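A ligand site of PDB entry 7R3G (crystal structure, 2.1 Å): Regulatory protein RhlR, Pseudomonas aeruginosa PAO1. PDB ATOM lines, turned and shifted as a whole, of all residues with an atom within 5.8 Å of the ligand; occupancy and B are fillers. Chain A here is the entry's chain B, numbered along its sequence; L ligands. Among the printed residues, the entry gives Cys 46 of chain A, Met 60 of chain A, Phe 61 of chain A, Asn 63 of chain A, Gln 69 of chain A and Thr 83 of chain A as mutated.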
ATOM      1  N   ALA A  44      22.355 -15.260  20.393  1.00  0.00           N
ATOM      2  CA  ALA A  44      22.978 -16.570  20.477  1.00  0.00           C
ATOM      3  C   ALA A  44      24.472 -16.408  20.228  1.00  0.00           C
ATOM      4  O   ALA A  44      24.900 -15.528  19.474  1.00  0.00           O
ATOM      5  CB  ALA A  44      22.366 -17.539  19.468  1.00  0.00           C
ATOM      6  N   TYR A  45      25.266 -17.243  20.901  1.00  0.00           N
ATOM      7  CA  TYR A  45      26.703 -17.322  20.666  1.00  0.00           C
ATOM      8  C   TYR A  45      27.050 -18.782  20.413  1.00  0.00           C
ATOM      9  O   TYR A  45      26.704 -19.649  21.213  1.00  0.00           O
ATOM     10  CB  TYR A  45      27.498 -16.788  21.855  1.00  0.00           C
ATOM     11  CG  TYR A  45      28.993 -16.909  21.698  1.00  0.00           C
ATOM     12  CD1 TYR A  45      29.628 -16.387  20.587  1.00  0.00           C
ATOM     13  CD2 TYR A  45      29.759 -17.558  22.646  1.00  0.00           C
ATOM     14  CE1 TYR A  45      31.009 -16.504  20.423  1.00  0.00           C
ATOM     15  CE2 TYR A  45      31.135 -17.684  22.505  1.00  0.00           C
ATOM     16  CZ  TYR A  45      31.751 -17.152  21.394  1.00  0.00           C
ATOM     17  OH  TYR A  45      33.115 -17.271  21.248  1.00  0.00           O
ATOM     18  N   CYS A  46      27.725 -19.050  19.286  1.00  0.00           N
ATOM     19  CA  CYS A  46      28.060 -20.402  18.863  1.00  0.00           C
ATOM     20  C   CYS A  46      29.558 -20.502  18.620  1.00  0.00           C
ATOM     21  O   CYS A  46      30.132 -19.642  17.944  1.00  0.00           O
ATOM     22  CB  CYS A  46      27.293 -20.793  17.583  1.00  0.00           C
ATOM     23  SG  CYS A  46      27.898 -22.243  16.644  1.00  0.00           S
ATOM     24  N   MET A  60      26.789 -24.156  21.836  1.00  0.00           N
ATOM     25  CA  MET A  60      25.785 -23.131  21.584  1.00  0.00           C
ATOM     26  C   MET A  60      25.332 -22.516  22.894  1.00  0.00           C
ATOM     27  O   MET A  60      25.116 -23.214  23.886  1.00  0.00           O
ATOM     28  CB  MET A  60      24.598 -23.717  20.829  1.00  0.00           C
ATOM     29  CG  MET A  60      25.004 -24.318  19.488  1.00  0.00           C
ATOM     30  SD  MET A  60      23.593 -24.810  18.484  1.00  0.00           S
ATOM     31  CE  MET A  60      23.503 -23.409  17.380  1.00  0.00           C
ATOM     32  N   PHE A  61      25.212 -21.187  22.886  1.00  0.00           N
ATOM     33  CA  PHE A  61      24.761 -20.427  24.038  1.00  0.00           C
ATOM     34  C   PHE A  61      23.774 -19.378  23.541  1.00  0.00           C
ATOM     35  O   PHE A  61      23.675 -19.091  22.348  1.00  0.00           O
ATOM     36  CB  PHE A  61      25.918 -19.735  24.774  1.00  0.00           C
ATOM     37  CG  PHE A  61      27.076 -20.637  25.098  1.00  0.00           C
ATOM     38  CD1 PHE A  61      28.079 -20.851  24.175  1.00  0.00           C
ATOM     39  CD2 PHE A  61      27.162 -21.256  26.333  1.00  0.00           C
ATOM     40  CE1 PHE A  61      29.148 -21.673  24.466  1.00  0.00           C
ATOM     41  CE2 PHE A  61      28.230 -22.089  26.633  1.00  0.00           C
ATOM     42  CZ  PHE A  61      29.234 -22.292  25.702  1.00  0.00           C
ATOM     43  N   GLY A  62      23.045 -18.788  24.485  1.00  0.00           N
ATOM     44  CA  GLY A  62      22.131 -17.720  24.150  1.00  0.00           C
ATOM     45  C   GLY A  62      20.868 -17.743  24.964  1.00  0.00           C
ATOM     46  O   GLY A  62      20.702 -18.591  25.845  1.00  0.00           O
ATOM     47  N   ASN A  63      19.966 -16.806  24.683  1.00  0.00           N
ATOM     48  CA  ASN A  63      18.704 -16.705  25.402  1.00  0.00           C
ATOM     49  C   ASN A  63      17.515 -16.725  24.464  1.00  0.00           C
ATOM     50  O   ASN A  63      16.452 -16.199  24.815  1.00  0.00           O
ATOM     51  CB  ASN A  63      18.690 -15.441  26.268  1.00  0.00           C
ATOM     52  CG  ASN A  63      18.751 -14.176  25.436  1.00  0.00           C
ATOM     53  OD1 ASN A  63      18.860 -14.224  24.212  1.00  0.00           O
ATOM     54  ND2 ASN A  63      18.690 -13.034  26.106  1.00  0.00           N
ATOM     55  N   TYR A  64      17.668 -17.284  23.262  1.00  0.00           N
ATOM     56  CA  TYR A  64      16.497 -17.573  22.434  1.00  0.00           C
ATOM     57  C   TYR A  64      15.443 -18.236  23.305  1.00  0.00           C
ATOM     58  O   TYR A  64      15.796 -18.951  24.249  1.00  0.00           O
ATOM     59  CB  TYR A  64      16.839 -18.513  21.278  1.00  0.00           C
ATOM     60  CG  TYR A  64      17.535 -17.876  20.099  1.00  0.00           C
ATOM     61  CD1 TYR A  64      17.350 -16.537  19.778  1.00  0.00           C
ATOM     62  CD2 TYR A  64      18.379 -18.628  19.291  1.00  0.00           C
ATOM     63  CE1 TYR A  64      17.987 -15.971  18.698  1.00  0.00           C
ATOM     64  CE2 TYR A  64      19.028 -18.068  18.216  1.00  0.00           C
ATOM     65  CZ  TYR A  64      18.826 -16.742  17.921  1.00  0.00           C
ATOM     66  OH  TYR A  64      19.459 -16.185  16.841  1.00  0.00           O
ATOM     67  N   TRP A  68      12.034 -22.290  21.029  1.00  0.00           N
ATOM     68  CA  TRP A  68      12.774 -22.254  19.775  1.00  0.00           C
ATOM     69  C   TRP A  68      14.054 -23.085  19.885  1.00  0.00           C
ATOM     70  O   TRP A  68      14.378 -23.857  18.973  1.00  0.00           O
ATOM     71  CB  TRP A  68      13.104 -20.823  19.365  1.00  0.00           C
ATOM     72  CG  TRP A  68      13.980 -20.768  18.157  1.00  0.00           C
ATOM     73  CD1 TRP A  68      15.258 -20.299  18.091  1.00  0.00           C
ATOM     74  CD2 TRP A  68      13.647 -21.206  16.824  1.00  0.00           C
ATOM     75  NE1 TRP A  68      15.752 -20.415  16.809  1.00  0.00           N
ATOM     76  CE2 TRP A  68      14.776 -20.966  16.016  1.00  0.00           C
ATOM     77  CE3 TRP A  68      12.509 -21.772  16.253  1.00  0.00           C
ATOM     78  CZ2 TRP A  68      14.800 -21.276  14.659  1.00  0.00           C
ATOM     79  CZ3 TRP A  68      12.533 -22.082  14.896  1.00  0.00           C
ATOM     80  CH2 TRP A  68      13.670 -21.835  14.119  1.00  0.00           C
ATOM     81  N   GLN A  69      14.777 -22.966  21.001  1.00  0.00           N
ATOM     82  CA  GLN A  69      15.983 -23.770  21.204  1.00  0.00           C
ATOM     83  C   GLN A  69      15.712 -25.243  20.958  1.00  0.00           C
ATOM     84  O   GLN A  69      16.450 -25.916  20.224  1.00  0.00           O
ATOM     85  CB  GLN A  69      16.508 -23.579  22.621  1.00  0.00           C
ATOM     86  CG  GLN A  69      17.055 -22.205  22.915  1.00  0.00           C
ATOM     87  CD  GLN A  69      17.873 -22.169  24.194  1.00  0.00           C
ATOM     88  OE1 GLN A  69      18.586 -23.120  24.509  1.00  0.00           O
ATOM     89  NE2 GLN A  69      17.771 -21.074  24.926  1.00  0.00           N
ATOM     90  N   TYR A  72      14.762 -25.951  17.286  1.00  0.00           N
ATOM     91  CA  TYR A  72      15.976 -25.857  16.475  1.00  0.00           C
ATOM     92  C   TYR A  72      16.810 -27.121  16.601  1.00  0.00           C
ATOM     93  O   TYR A  72      17.268 -27.681  15.591  1.00  0.00           O
ATOM     94  CB  TYR A  72      16.766 -24.622  16.912  1.00  0.00           C
ATOM     95  CG  TYR A  72      17.977 -24.312  16.095  1.00  0.00           C
ATOM     96  CD1 TYR A  72      19.176 -24.976  16.332  1.00  0.00           C
ATOM     97  CD2 TYR A  72      17.948 -23.339  15.102  1.00  0.00           C
ATOM     98  CE1 TYR A  72      20.303 -24.690  15.590  1.00  0.00           C
ATOM     99  CE2 TYR A  72      19.068 -23.048  14.365  1.00  0.00           C
ATOM    100  CZ  TYR A  72      20.244 -23.735  14.607  1.00  0.00           C
ATOM    101  OH  TYR A  72      21.370 -23.459  13.874  1.00  0.00           O
ATOM    102  N   GLN A  73      16.990 -27.619  17.824  1.00  0.00           N
ATOM    103  CA  GLN A  73      17.778 -28.824  18.016  1.00  0.00           C
ATOM    104  C   GLN A  73      17.059 -30.052  17.473  1.00  0.00           C
ATOM    105  O   GLN A  73      17.674 -30.908  16.829  1.00  0.00           O
ATOM    106  CB  GLN A  73      18.105 -29.004  19.501  1.00  0.00           C
ATOM    107  CG  GLN A  73      19.196 -28.052  20.002  1.00  0.00           C
ATOM    108  CD  GLN A  73      18.952 -27.592  21.431  1.00  0.00           C
ATOM    109  OE1 GLN A  73      18.259 -28.253  22.203  1.00  0.00           O
ATOM    110  NE2 GLN A  73      19.520 -26.444  21.777  1.00  0.00           N
ATOM    111  N   ASP A  81      21.906 -24.352   8.779  1.00  0.00           N
ATOM    112  CA  ASP A  81      21.758 -22.952   9.133  1.00  0.00           C
ATOM    113  C   ASP A  81      22.794 -22.109   8.399  1.00  0.00           C
ATOM    114  O   ASP A  81      23.989 -22.251   8.655  1.00  0.00           O
ATOM    115  CB  ASP A  81      21.899 -22.785  10.654  1.00  0.00           C
ATOM    116  CG  ASP A  81      21.424 -21.437  11.148  1.00  0.00           C
ATOM    117  OD1 ASP A  81      21.350 -20.485  10.348  1.00  0.00           O
ATOM    118  OD2 ASP A  81      21.126 -21.345  12.352  1.00  0.00           O
ATOM    119  N   THR A  83      23.589 -19.079   8.813  1.00  0.00           N
ATOM    120  CA  THR A  83      24.268 -18.101   9.640  1.00  0.00           C
ATOM    121  C   THR A  83      25.462 -18.683  10.386  1.00  0.00           C
ATOM    122  O   THR A  83      26.308 -17.918  10.872  1.00  0.00           O
ATOM    123  CB  THR A  83      23.311 -17.482  10.667  1.00  0.00           C
ATOM    124  OG1 THR A  83      22.885 -18.465  11.618  1.00  0.00           O
ATOM    125  CG2 THR A  83      22.092 -16.887   9.978  1.00  0.00           C
ATOM    126  N   ILE A  84      25.549 -19.994  10.523  1.00  0.00           N
ATOM    127  CA  ILE A  84      26.710 -20.592  11.179  1.00  0.00           C
ATOM    128  C   ILE A  84      27.486 -21.489  10.224  1.00  0.00           C
ATOM    129  O   ILE A  84      28.188 -22.388  10.655  1.00  0.00           O
ATOM    130  CB  ILE A  84      26.308 -21.349  12.460  1.00  0.00           C
ATOM    131  CG1 ILE A  84      25.207 -22.364  12.184  1.00  0.00           C
ATOM    132  CG2 ILE A  84      25.872 -20.360  13.535  1.00  0.00           C
ATOM    133  CD1 ILE A  84      25.148 -23.494  13.212  1.00  0.00           C
ATOM    134  N   TRP A  96      19.912 -10.760   8.461  1.00  0.00           N
ATOM    135  CA  TRP A  96      19.011 -11.812   8.013  1.00  0.00           C
ATOM    136  C   TRP A  96      18.066 -11.295   6.934  1.00  0.00           C
ATOM    137  O   TRP A  96      17.602 -10.158   6.987  1.00  0.00           O
ATOM    138  CB  TRP A  96      18.210 -12.360   9.189  1.00  0.00           C
ATOM    139  CG  TRP A  96      19.043 -12.954  10.276  1.00  0.00           C
ATOM    140  CD1 TRP A  96      20.399 -13.125  10.279  1.00  0.00           C
ATOM    141  CD2 TRP A  96      18.572 -13.449  11.523  1.00  0.00           C
ATOM    142  NE1 TRP A  96      20.803 -13.696  11.455  1.00  0.00           N
ATOM    143  CE2 TRP A  96      19.696 -13.914  12.236  1.00  0.00           C
ATOM    144  CE3 TRP A  96      17.307 -13.561  12.119  1.00  0.00           C
ATOM    145  CZ2 TRP A  96      19.598 -14.469  13.510  1.00  0.00           C
ATOM    146  CZ3 TRP A  96      17.209 -14.105  13.383  1.00  0.00           C
ATOM    147  CH2 TRP A  96      18.346 -14.555  14.061  1.00  0.00           C
ATOM    148  N   PHE A 101      18.161 -17.253   3.441  1.00  0.00           N
ATOM    149  CA  PHE A 101      17.580 -18.539   3.780  1.00  0.00           C
ATOM    150  C   PHE A 101      16.911 -19.219   2.593  1.00  0.00           C
ATOM    151  O   PHE A 101      16.113 -20.143   2.785  1.00  0.00           O
ATOM    152  CB  PHE A 101      16.580 -18.361   4.927  1.00  0.00           C
ATOM    153  CG  PHE A 101      17.205 -17.906   6.204  1.00  0.00           C
ATOM    154  CD1 PHE A 101      17.854 -18.811   7.023  1.00  0.00           C
ATOM    155  CD2 PHE A 101      17.167 -16.575   6.573  1.00  0.00           C
ATOM    156  CE1 PHE A 101      18.443 -18.407   8.194  1.00  0.00           C
ATOM    157  CE2 PHE A 101      17.761 -16.162   7.744  1.00  0.00           C
ATOM    158  CZ  PHE A 101      18.389 -17.078   8.558  1.00  0.00           C
ATOM    159  N   LEU A 107      13.748 -23.654   8.003  1.00  0.00           N
ATOM    160  CA  LEU A 107      14.335 -22.977   9.157  1.00  0.00           C
ATOM    161  C   LEU A 107      13.799 -21.553   9.283  1.00  0.00           C
ATOM    162  O   LEU A 107      13.414 -21.111  10.381  1.00  0.00           O
ATOM    163  CB  LEU A 107      15.854 -22.975   9.062  1.00  0.00           C
ATOM    164  CG  LEU A 107      16.636 -21.983   9.925  1.00  0.00           C
ATOM    165  CD1 LEU A 107      16.419 -22.249  11.414  1.00  0.00           C
ATOM    166  CD2 LEU A 107      18.116 -22.062   9.584  1.00  0.00           C
ATOM    167  N   TRP A 108      13.756 -20.821   8.177  1.00  0.00           N
ATOM    168  CA  TRP A 108      13.371 -19.409   8.224  1.00  0.00           C
ATOM    169  C   TRP A 108      11.882 -19.247   8.444  1.00  0.00           C
ATOM    170  O   TRP A 108      11.448 -18.350   9.175  1.00  0.00           O
ATOM    171  CB  TRP A 108      13.822 -18.723   6.940  1.00  0.00           C
ATOM    172  CG  TRP A 108      13.682 -17.226   6.868  1.00  0.00           C
ATOM    173  CD1 TRP A 108      13.248 -16.514   5.802  1.00  0.00           C
ATOM    174  CD2 TRP A 108      14.001 -16.273   7.888  1.00  0.00           C
ATOM    175  NE1 TRP A 108      13.270 -15.169   6.082  1.00  0.00           N
ATOM    176  CE2 TRP A 108      13.729 -15.000   7.356  1.00  0.00           C
ATOM    177  CE3 TRP A 108      14.492 -16.369   9.200  1.00  0.00           C
ATOM    178  CZ2 TRP A 108      13.923 -13.824   8.091  1.00  0.00           C
ATOM    179  CZ3 TRP A 108      14.685 -15.204   9.922  1.00  0.00           C
ATOM    180  CH2 TRP A 108      14.400 -13.947   9.358  1.00  0.00           C
ATOM    181  N   ALA A 111      11.500 -20.087  12.186  1.00  0.00           N
ATOM    182  CA  ALA A 111      12.054 -19.021  13.019  1.00  0.00           C
ATOM    183  C   ALA A 111      11.094 -17.837  13.107  1.00  0.00           C
ATOM    184  O   ALA A 111      10.868 -17.286  14.183  1.00  0.00           O
ATOM    185  CB  ALA A 111      13.406 -18.581  12.471  1.00  0.00           C
ATOM    186  N   LEU A 116      11.197 -14.766  15.615  1.00  0.00           N
ATOM    187  CA  LEU A 116      12.561 -14.355  15.277  1.00  0.00           C
ATOM    188  C   LEU A 116      12.532 -13.903  13.824  1.00  0.00           C
ATOM    189  O   LEU A 116      12.817 -14.665  12.899  1.00  0.00           O
ATOM    190  CB  LEU A 116      13.528 -15.507  15.494  1.00  0.00           C
ATOM    191  CG  LEU A 116      13.415 -16.202  16.853  1.00  0.00           C
ATOM    192  CD1 LEU A 116      14.276 -17.446  16.917  1.00  0.00           C
ATOM    193  CD2 LEU A 116      13.796 -15.236  17.950  1.00  0.00           C
ATOM    194  N   THR A 121      23.915 -11.751  12.076  1.00  0.00           N
ATOM    195  CA  THR A 121      24.937 -12.626  12.631  1.00  0.00           C
ATOM    196  C   THR A 121      26.302 -12.080  12.256  1.00  0.00           C
ATOM    197  O   THR A 121      26.548 -11.760  11.089  1.00  0.00           O
ATOM    198  CB  THR A 121      24.789 -14.064  12.140  1.00  0.00           C
ATOM    199  OG1 THR A 121      23.470 -14.544  12.465  1.00  0.00           O
ATOM    200  CG2 THR A 121      25.813 -14.963  12.788  1.00  0.00           C
ATOM    201  N   SER A 135      24.692 -13.955  17.138  1.00  0.00           N
ATOM    202  CA  SER A 135      23.423 -13.549  16.540  1.00  0.00           C
ATOM    203  C   SER A 135      22.642 -12.672  17.504  1.00  0.00           C
ATOM    204  O   SER A 135      22.686 -12.873  18.718  1.00  0.00           O
ATOM    205  CB  SER A 135      22.576 -14.765  16.165  1.00  0.00           C
ATOM    206  OG  SER A 135      23.191 -15.509  15.135  1.00  0.00           O
HETATM  207 BR1  LIG L   1      21.113 -21.810  22.928  1.00  0.00          BR
HETATM  208  C1  LIG L   1      20.768 -21.972  21.074  1.00  0.00           C
HETATM  209  C2  LIG L   1      21.520 -21.240  20.182  1.00  0.00           C
HETATM  210  C3  LIG L   1      21.273 -21.373  18.825  1.00  0.00           C
HETATM  211  C4  LIG L   1      20.267 -22.212  18.370  1.00  0.00           C
HETATM  212  C5  LIG L   1      19.519 -22.935  19.284  1.00  0.00           C
HETATM  213  C6  LIG L   1      19.769 -22.825  20.646  1.00  0.00           C
HETATM  214  O1  LIG L   1      22.129 -20.662  18.028  1.00  0.00           O
HETATM  215  C7  LIG L   1      21.818 -20.524  16.637  1.00  0.00           C
HETATM  216  C8  LIG L   1      22.989 -19.774  16.058  1.00  0.00           C
HETATM  217  C9  LIG L   1      22.718 -19.341  14.638  1.00  0.00           C
HETATM  218  C10 LIG L   1      21.477 -18.485  14.551  1.00  0.00           C
HETATM  219  O2  LIG L   1      21.356 -17.448  15.190  1.00  0.00           O
HETATM  220  N1  LIG L   1      20.507 -18.948  13.753  1.00  0.00           N
HETATM  221  C11 LIG L   1      19.312 -18.162  13.496  1.00  0.00           C
HETATM  222  C12 LIG L   1      18.828 -18.182  12.033  1.00  0.00           C
HETATM  223  C13 LIG L   1      17.454 -17.526  12.058  1.00  0.00           C
HETATM  224  S1  LIG L   1      16.635 -18.108  13.579  1.00  0.00           S
HETATM  225  C14 LIG L   1      18.133 -18.680  14.298  1.00  0.00           C
HETATM  226  O3  LIG L   1      18.197 -19.367  15.283  1.00  0.00           O
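O of Ala 44 sits at hydrogen-bond distance from N of Ser 135.
The side-chain hydroxyl of Thr 121 is in hydrogen-bond range of the side-chain hydroxyl of Ser 135, at 2.9 Å.
The backbone carbonyl oxygen (O) of Tyr 64 lies within hydrogen-bond range of the side-chain amide nitrogen (NE2) of Gln 69, at 3.0 Å.
The side-chain hydroxyl (OG1) of Thr 83 lies within hydrogen-bond range of the side-chain carboxylate (OD1) of Asp 81 (2.8 Å).
OD2 of Asp 81 lies within hydrogen-bond range of OH of Tyr 72 (2.6 Å).
O of Gln 69 lies close to NE2 of Gln 73.
The backbone NH (N) of Leu 116 is in hydrogen-bond range of the backbone carbonyl oxygen (O) of Ala 111, at 2.9 Å.
NE1 of Trp 96 sits at hydrogen-bond distance from OG1 of Thr 121, at 3.0 Å.
OG of Ser 135 is in hydrogen-bond range of O2 of the ligand (2.7 Å).
The side-chain hydroxyl (OH) of Tyr 64 lies within hydrogen-bond range of an oxygen (O2) of the ligand, 2.8 Å away.
The side-chain carboxylate of Asp 81 lies within hydrogen-bond range of a nitrogen (N1) of the ligand (2.8 Å).
The indole nitrogen (NE1) of Trp 68 sits at hydrogen-bond distance from an oxygen (O3) of the ligand, at 3.1 Å.
The side-chain hydroxyl of Thr 83 sits close to a nitrogen (N1) of the ligand (3.2 Å).
Merely in contact with the ligand: Met 60 (3.1 Å), Gln 69 (3.3 Å), Ala 111 (3.4 Å), Ala 44 (3.4 Å), Ile 84 (3.5 Å), Tyr 72 (3.6 Å), Phe 101 (3.7 Å), Phe 61 (3.7 Å), Trp 96 (3.7 Å), Gln 73 (3.8 Å) and Gly 62 (3.9 Å).
Hydrophobic or aromatic side chains within 4 Å of the ligand: Ala 44, Met 60, Tyr 64, Trp 68, Tyr 72, Ile 84, Trp 96, Phe 101 and Ala 111.
16 residues have an atom within 4 Å of the ligand: Ala 44, Met 60, Phe 61, Gly 62, Tyr 64, Trp 68, Gln 69, Tyr 72, Gln 73, Asp 81, Thr 83, Ile 84, Trp 96, Phe 101, Ala 111 and Ser 135.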
